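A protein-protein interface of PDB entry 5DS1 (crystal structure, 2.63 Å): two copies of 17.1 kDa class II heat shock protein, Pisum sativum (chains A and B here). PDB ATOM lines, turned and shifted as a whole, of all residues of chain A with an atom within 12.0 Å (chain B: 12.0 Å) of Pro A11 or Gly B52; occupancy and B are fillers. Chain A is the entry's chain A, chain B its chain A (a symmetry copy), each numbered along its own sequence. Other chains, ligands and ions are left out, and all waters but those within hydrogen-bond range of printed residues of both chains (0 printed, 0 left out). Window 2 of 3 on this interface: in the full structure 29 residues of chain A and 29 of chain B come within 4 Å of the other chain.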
ATOM      1  N   VAL A   7      27.141  18.785   2.869  1.00  0.00           N
ATOM      2  CA  VAL A   7      27.117  19.644   1.687  1.00  0.00           C
ATOM      3  C   VAL A   7      27.177  18.760   0.448  1.00  0.00           C
ATOM      4  O   VAL A   7      28.134  17.996   0.274  1.00  0.00           O
ATOM      5  CB  VAL A   7      28.276  20.655   1.680  1.00  0.00           C
ATOM      6  CG1 VAL A   7      28.080  21.665   0.585  1.00  0.00           C
ATOM      7  CG2 VAL A   7      28.398  21.358   3.045  1.00  0.00           C
ATOM      8  N   LYS A   8      26.170  18.866  -0.417  1.00  0.00           N
ATOM      9  CA  LYS A   8      26.087  18.068  -1.638  1.00  0.00           C
ATOM     10  C   LYS A   8      26.103  18.980  -2.859  1.00  0.00           C
ATOM     11  O   LYS A   8      25.758  20.161  -2.781  1.00  0.00           O
ATOM     12  CB  LYS A   8      24.820  17.184  -1.665  1.00  0.00           C
ATOM     13  CG  LYS A   8      24.655  16.243  -0.472  1.00  0.00           C
ATOM     14  CD  LYS A   8      23.445  15.331  -0.630  1.00  0.00           C
ATOM     15  CE  LYS A   8      22.145  16.081  -0.406  1.00  0.00           C
ATOM     16  NZ  LYS A   8      21.326  16.230  -1.660  1.00  0.00           N
ATOM     17  N   GLU A   9      26.515  18.420  -3.998  1.00  0.00           N
ATOM     18  CA  GLU A   9      26.611  19.149  -5.263  1.00  0.00           C
ATOM     19  C   GLU A   9      25.715  18.472  -6.299  1.00  0.00           C
ATOM     20  O   GLU A   9      26.063  17.421  -6.848  1.00  0.00           O
ATOM     21  CB  GLU A   9      28.059  19.226  -5.768  1.00  0.00           C
ATOM     22  CG  GLU A   9      28.183  19.651  -7.267  1.00  0.00           C
ATOM     23  CD  GLU A   9      29.552  20.231  -7.652  1.00  0.00           C
ATOM     24  OE1 GLU A   9      30.328  20.596  -6.753  1.00  0.00           O
ATOM     25  OE2 GLU A   9      29.842  20.281  -8.861  1.00  0.00           O
ATOM     26  N   HIS A  10      24.581  19.085  -6.580  1.00  0.00           N
ATOM     27  CA  HIS A  10      23.707  18.647  -7.657  1.00  0.00           C
ATOM     28  C   HIS A  10      24.152  19.279  -8.960  1.00  0.00           C
ATOM     29  O   HIS A  10      25.035  20.138  -8.966  1.00  0.00           O
ATOM     30  CB  HIS A  10      22.264  19.000  -7.312  1.00  0.00           C
ATOM     31  CG  HIS A  10      21.809  18.411  -6.016  1.00  0.00           C
ATOM     32  ND1 HIS A  10      21.014  17.287  -5.945  1.00  0.00           N
ATOM     33  CD2 HIS A  10      22.043  18.789  -4.738  1.00  0.00           C
ATOM     34  CE1 HIS A  10      20.774  17.000  -4.678  1.00  0.00           C
ATOM     35  NE2 HIS A  10      21.380  17.900  -3.926  1.00  0.00           N
ATOM     36  N   PRO A  11      23.596  18.836 -10.095  1.00  0.00           N
ATOM     37  CA  PRO A  11      24.043  19.390 -11.391  1.00  0.00           C
ATOM     38  C   PRO A  11      24.110  20.911 -11.449  1.00  0.00           C
ATOM     39  O   PRO A  11      25.117  21.468 -11.912  1.00  0.00           O
ATOM     40  CB  PRO A  11      23.003  18.819 -12.363  1.00  0.00           C
ATOM     41  CG  PRO A  11      22.689  17.476 -11.794  1.00  0.00           C
ATOM     42  CD  PRO A  11      22.716  17.662 -10.285  1.00  0.00           C
ATOM     43  N   ASN A  12      23.082  21.600 -10.950  1.00  0.00           N
ATOM     44  CA  ASN A  12      22.975  23.049 -11.082  1.00  0.00           C
ATOM     45  C   ASN A  12      22.843  23.757  -9.738  1.00  0.00           C
ATOM     46  O   ASN A  12      22.383  24.906  -9.693  1.00  0.00           O
ATOM     47  CB  ASN A  12      21.783  23.404 -11.969  1.00  0.00           C
ATOM     48  CG  ASN A  12      21.613  22.438 -13.116  1.00  0.00           C
ATOM     49  OD1 ASN A  12      22.398  22.437 -14.062  1.00  0.00           O
ATOM     50  ND2 ASN A  12      20.586  21.594 -13.033  1.00  0.00           N
ATOM     51  N   SER A  13      23.248  23.116  -8.642  1.00  0.00           N
ATOM     52  CA  SER A  13      22.989  23.693  -7.329  1.00  0.00           C
ATOM     53  C   SER A  13      23.874  23.039  -6.278  1.00  0.00           C
ATOM     54  O   SER A  13      24.318  21.894  -6.424  1.00  0.00           O
ATOM     55  CB  SER A  13      21.513  23.542  -6.932  1.00  0.00           C
ATOM     56  OG  SER A  13      21.224  22.196  -6.618  1.00  0.00           O
ATOM     57  N   TYR A  14      24.095  23.782  -5.199  1.00  0.00           N
ATOM     58  CA  TYR A  14      24.726  23.284  -3.988  1.00  0.00           C
ATOM     59  C   TYR A  14      23.699  23.200  -2.860  1.00  0.00           C
ATOM     60  O   TYR A  14      22.812  24.055  -2.756  1.00  0.00           O
ATOM     61  CB  TYR A  14      25.856  24.209  -3.578  1.00  0.00           C
ATOM     62  CG  TYR A  14      26.943  24.373  -4.597  1.00  0.00           C
ATOM     63  CD1 TYR A  14      27.895  23.362  -4.810  1.00  0.00           C
ATOM     64  CD2 TYR A  14      27.050  25.547  -5.326  1.00  0.00           C
ATOM     65  CE1 TYR A  14      28.913  23.529  -5.730  1.00  0.00           C
ATOM     66  CE2 TYR A  14      28.064  25.723  -6.240  1.00  0.00           C
ATOM     67  CZ  TYR A  14      28.985  24.715  -6.439  1.00  0.00           C
ATOM     68  OH  TYR A  14      29.979  24.892  -7.357  1.00  0.00           O
ATOM     69  N   VAL A  15      23.820  22.183  -2.008  1.00  0.00           N
ATOM     70  CA  VAL A  15      22.852  21.931  -0.943  1.00  0.00           C
ATOM     71  C   VAL A  15      23.582  21.825   0.386  1.00  0.00           C
ATOM     72  O   VAL A  15      24.554  21.070   0.509  1.00  0.00           O
ATOM     73  CB  VAL A  15      22.037  20.654  -1.204  1.00  0.00           C
ATOM     74  CG1 VAL A  15      21.286  20.277   0.031  1.00  0.00           C
ATOM     75  CG2 VAL A  15      21.083  20.876  -2.356  1.00  0.00           C
ATOM     76  N   LEU A  71      31.378  29.772  -1.173  1.00  0.00           N
ATOM     77  CA  LEU A  71      31.442  29.250  -2.523  1.00  0.00           C
ATOM     78  C   LEU A  71      32.489  30.035  -3.289  1.00  0.00           C
ATOM     79  O   LEU A  71      32.905  31.105  -2.834  1.00  0.00           O
ATOM     80  CB  LEU A  71      30.070  29.366  -3.184  1.00  0.00           C
ATOM     81  CG  LEU A  71      28.910  28.720  -2.409  1.00  0.00           C
ATOM     82  CD1 LEU A  71      28.113  29.750  -1.599  1.00  0.00           C
ATOM     83  CD2 LEU A  71      28.011  27.940  -3.344  1.00  0.00           C
ATOM     84  N   PRO A  72      32.961  29.535  -4.438  1.00  0.00           N
ATOM     85  CA  PRO A  72      34.033  30.242  -5.163  1.00  0.00           C
ATOM     86  C   PRO A  72      33.689  31.698  -5.455  1.00  0.00           C
ATOM     87  O   PRO A  72      32.521  32.089  -5.504  1.00  0.00           O
ATOM     88  CB  PRO A  72      34.175  29.436  -6.462  1.00  0.00           C
ATOM     89  CG  PRO A  72      32.966  28.562  -6.529  1.00  0.00           C
ATOM     90  CD  PRO A  72      32.611  28.272  -5.105  1.00  0.00           C
ATOM     91  N   ALA A  75      31.095  33.447  -8.057  1.00  0.00           N
ATOM     92  CA  ALA A  75      29.909  32.590  -8.015  1.00  0.00           C
ATOM     93  C   ALA A  75      28.806  33.380  -7.322  1.00  0.00           C
ATOM     94  O   ALA A  75      28.783  33.493  -6.094  1.00  0.00           O
ATOM     95  CB  ALA A  75      30.204  31.275  -7.301  1.00  0.00           C
ATOM     96  N   THR A  92      19.383  25.291  -0.435  1.00  0.00           N
ATOM     97  CA  THR A  92      19.865  25.033  -1.784  1.00  0.00           C
ATOM     98  C   THR A  92      20.177  26.354  -2.465  1.00  0.00           C
ATOM     99  O   THR A  92      19.292  27.194  -2.638  1.00  0.00           O
ATOM    100  CB  THR A  92      18.840  24.245  -2.596  1.00  0.00           C
ATOM    101  OG1 THR A  92      18.661  22.967  -1.978  1.00  0.00           O
ATOM    102  CG2 THR A  92      19.274  24.114  -4.057  1.00  0.00           C
ATOM    103  N   VAL A  93      21.420  26.511  -2.887  1.00  0.00           N
ATOM    104  CA  VAL A  93      21.943  27.755  -3.441  1.00  0.00           C
ATOM    105  C   VAL A  93      22.378  27.468  -4.874  1.00  0.00           C
ATOM    106  O   VAL A  93      23.048  26.463  -5.135  1.00  0.00           O
ATOM    107  CB  VAL A  93      23.103  28.275  -2.560  1.00  0.00           C
ATOM    108  CG1 VAL A  93      24.362  28.440  -3.326  1.00  0.00           C
ATOM    109  CG2 VAL A  93      22.747  29.567  -1.893  1.00  0.00           C
ATOM    110  N   ASN A  94      21.946  28.298  -5.813  1.00  0.00           N
ATOM    111  CA  ASN A  94      22.524  28.253  -7.173  1.00  0.00           C
ATOM    112  C   ASN A  94      24.033  28.443  -7.096  1.00  0.00           C
ATOM    113  O   ASN A  94      24.788  27.731  -7.742  1.00  0.00           O
ATOM    114  CB  ASN A  94      21.940  29.343  -8.073  1.00  0.00           C
ATOM    115  CG  ASN A  94      22.625  30.681  -7.855  1.00  0.00           C
ATOM    116  OD1 ASN A  94      22.350  31.375  -6.862  1.00  0.00           O
ATOM    117  ND2 ASN A  94      23.543  31.043  -8.761  1.00  0.00           N
ATOM    118  N   ARG B  46      19.918   8.411   5.519  1.00  0.00           N
ATOM    119  CA  ARG B  46      20.436   9.168   4.388  1.00  0.00           C
ATOM    120  C   ARG B  46      19.385   9.295   3.289  1.00  0.00           C
ATOM    121  O   ARG B  46      18.600   8.376   3.037  1.00  0.00           O
ATOM    122  CB  ARG B  46      21.683   8.493   3.813  1.00  0.00           C
ATOM    123  CG  ARG B  46      21.462   7.852   2.437  1.00  0.00           C
ATOM    124  CD  ARG B  46      22.691   7.116   1.928  1.00  0.00           C
ATOM    125  NE  ARG B  46      22.679   6.914   0.477  1.00  0.00           N
ATOM    126  CZ  ARG B  46      22.181   5.840  -0.132  1.00  0.00           C
ATOM    127  NH1 ARG B  46      22.227   5.745  -1.457  1.00  0.00           N
ATOM    128  NH2 ARG B  46      21.631   4.864   0.582  1.00  0.00           N
ATOM    129  N   GLU B  47      19.372  10.452   2.633  1.00  0.00           N
ATOM    130  CA  GLU B  47      18.588  10.631   1.413  1.00  0.00           C
ATOM    131  C   GLU B  47      19.423  10.079   0.261  1.00  0.00           C
ATOM    132  O   GLU B  47      20.300  10.754  -0.277  1.00  0.00           O
ATOM    133  CB  GLU B  47      18.218  12.095   1.210  1.00  0.00           C
ATOM    134  N   GLU B  48      19.162   8.822  -0.097  1.00  0.00           N
ATOM    135  CA  GLU B  48      19.810   8.174  -1.232  1.00  0.00           C
ATOM    136  C   GLU B  48      19.598   8.971  -2.524  1.00  0.00           C
ATOM    137  O   GLU B  48      20.498   9.083  -3.364  1.00  0.00           O
ATOM    138  CB  GLU B  48      19.278   6.747  -1.406  1.00  0.00           C
ATOM    139  N   LYS B  50      24.384   8.271  -6.215  1.00  0.00           N
ATOM    140  CA  LYS B  50      24.999   9.323  -7.025  1.00  0.00           C
ATOM    141  C   LYS B  50      24.188   9.605  -8.292  1.00  0.00           C
ATOM    142  O   LYS B  50      24.563   9.174  -9.388  1.00  0.00           O
ATOM    143  CB  LYS B  50      26.434   8.945  -7.403  1.00  0.00           C
ATOM    144  N   GLU B  51      23.040  10.255  -8.166  1.00  0.00           N
ATOM    145  CA  GLU B  51      22.207  10.509  -9.332  1.00  0.00           C
ATOM    146  C   GLU B  51      22.747  11.750  -9.973  1.00  0.00           C
ATOM    147  O   GLU B  51      22.015  12.609 -10.418  1.00  0.00           O
ATOM    148  CB  GLU B  51      20.760  10.727  -8.904  1.00  0.00           C
ATOM    149  N   GLY B  52      24.059  11.825 -10.007  1.00  0.00           N
ATOM    150  CA  GLY B  52      24.732  13.007 -10.474  1.00  0.00           C
ATOM    151  C   GLY B  52      24.913  13.923  -9.266  1.00  0.00           C
ATOM    152  O   GLY B  52      25.238  15.086  -9.412  1.00  0.00           O
ATOM    153  N   VAL B  53      24.692  13.386  -8.068  1.00  0.00           N
ATOM    154  CA  VAL B  53      24.819  14.096  -6.827  1.00  0.00           C
ATOM    155  C   VAL B  53      26.017  13.560  -6.099  1.00  0.00           C
ATOM    156  O   VAL B  53      26.125  12.398  -5.834  1.00  0.00           O
ATOM    157  CB  VAL B  53      23.602  13.884  -5.942  1.00  0.00           C
ATOM    158  CG1 VAL B  53      23.622  14.858  -4.789  1.00  0.00           C
ATOM    159  CG2 VAL B  53      22.341  14.017  -6.761  1.00  0.00           C
ATOM    160  N   LYS B  54      26.913  14.451  -5.781  1.00  0.00           N
ATOM    161  CA  LYS B  54      28.148  14.126  -5.081  1.00  0.00           C
ATOM    162  C   LYS B  54      28.226  14.907  -3.773  1.00  0.00           C
ATOM    163  O   LYS B  54      27.913  16.100  -3.729  1.00  0.00           O
ATOM    164  CB  LYS B  54      29.386  14.418  -5.955  1.00  0.00           C
ATOM    165  CG  LYS B  54      29.262  15.630  -6.872  1.00  0.00           C
ATOM    166  CD  LYS B  54      30.189  15.518  -8.102  1.00  0.00           C
ATOM    167  CE  LYS B  54      29.772  16.458  -9.241  1.00  0.00           C
ATOM    168  NZ  LYS B  54      28.604  15.948 -10.025  1.00  0.00           N
ATOM    169  N   TYR B  55      28.632  14.224  -2.703  1.00  0.00           N
ATOM    170  CA  TYR B  55      28.849  14.870  -1.413  1.00  0.00           C
ATOM    171  C   TYR B  55      30.159  15.642  -1.411  1.00  0.00           C
ATOM    172  O   TYR B  55      31.200  15.108  -1.804  1.00  0.00           O
ATOM    173  CB  TYR B  55      28.880  13.826  -0.301  1.00  0.00           C
ATOM    174  CG  TYR B  55      27.541  13.537   0.287  1.00  0.00           C
ATOM    175  CD1 TYR B  55      27.049  14.306   1.327  1.00  0.00           C
ATOM    176  CD2 TYR B  55      26.757  12.496  -0.190  1.00  0.00           C
ATOM    177  CE1 TYR B  55      25.801  14.044   1.889  1.00  0.00           C
ATOM    178  CE2 TYR B  55      25.501  12.231   0.367  1.00  0.00           C
ATOM    179  CZ  TYR B  55      25.038  13.014   1.397  1.00  0.00           C
ATOM    180  OH  TYR B  55      23.810  12.768   1.954  1.00  0.00           O
ATOM    181  N   LEU B  56      30.126  16.888  -0.946  1.00  0.00           N
ATOM    182  CA  LEU B  56      31.388  17.592  -0.718  1.00  0.00           C
ATOM    183  C   LEU B  56      31.811  17.573   0.739  1.00  0.00           C
ATOM    184  O   LEU B  56      33.009  17.532   1.032  1.00  0.00           O
ATOM    185  CB  LEU B  56      31.316  19.046  -1.202  1.00  0.00           C
ATOM    186  CG  LEU B  56      30.700  19.282  -2.571  1.00  0.00           C
ATOM    187  CD1 LEU B  56      30.875  20.707  -2.986  1.00  0.00           C
ATOM    188  CD2 LEU B  56      31.311  18.372  -3.603  1.00  0.00           C
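NZ of Lys A8 lies within hydrogen-bond range of NE2 of His A10, at 2.8 Å.
The backbone carbonyl oxygen (O) of Val A15 sits at hydrogen-bond distance from the backbone NH (N) of Lys A8 (2.9 Å).
No position is printed for both chains.
Pro A11 touches just one residue of chain B: Gly B52.
Glu A9 touches four residues of chain B.
Of chain B, only Val B53 comes within 4 Å of His A10.
No residue of chain B comes within 4 Å of Asn A12.
No residue of chain B comes within 4 Å of Ser A13.
No residue of chain A comes within 4 Å of Glu B51.
Val B53 touches two residues of chain A.
Lys B54 touches just these residues of chain A: Lys A8 and Glu A9.
Printed residues of chain B within 4 Å of Val A7: Tyr B55 (3.5 Å) and Leu B56 (2.6 Å).
Of the printed residues of chain A, Leu B56 touches Val A7 and Glu A9.
Printed residues of chain B within 4 Å of Lys A8: Lys B54 and Tyr B55.
Of the printed residues of chain A, Tyr B55 touches Val A7 (3.5 Å) and Lys A8 (3.4 Å).
Pro A72 touches none of the printed residues of chain B.
Arg B46 touches none of the printed residues of chain A.
The nearest printed residue of chain B that does not touch Pro A11 is Val B53 (5.1 Å).
The nearest printed residue of chain B that does not touch Lys A8 is Val B53 (4.1 Å).
The backbone NH of Glu A9 is in hydrogen-bond range of the backbone carbonyl oxygen of Lys B54 (2.7 Å).
The backbone carbonyl oxygen (O) of Val A7 lies within hydrogen-bond range of the backbone NH (N) of Leu B56, 2.6 Å away.
Hydrophobic or aromatic side chains of chain B that line the printed part of chain A: Val B53, Tyr B55 and Leu B56.
Of the 15 printed residues of chain A, 5 touch a printed residue of chain B.
Hydrophobic or aromatic side chains of chain A within 4 Å of the printed part of chain B: His A10 and Pro A11.
Among the printed residues, 10 pairs touch across the chains.
Among the printed residues, no Asp or Glu carboxylate lies within 4 Å of a Lys or Arg side-chain nitrogen of the other chain.
Val A7 touches Tyr B55 (O to C, 3.5 Å).
O of Lys B54 touches CA of Lys A8, 3.4 Å away.
CG of Lys A8 touches CE1 of Tyr B55 (3.4 Å).
O of Glu A9 touches O of Gly B52, 3.6 Å away.
Glu A9 touches Val B53.
Glu A9 touches Leu B56 (OE1 to CD1, 3.8 Å).
Val B53 touches His A10.
CD of Pro A11 touches O of Gly B52, 3.7 Å away.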
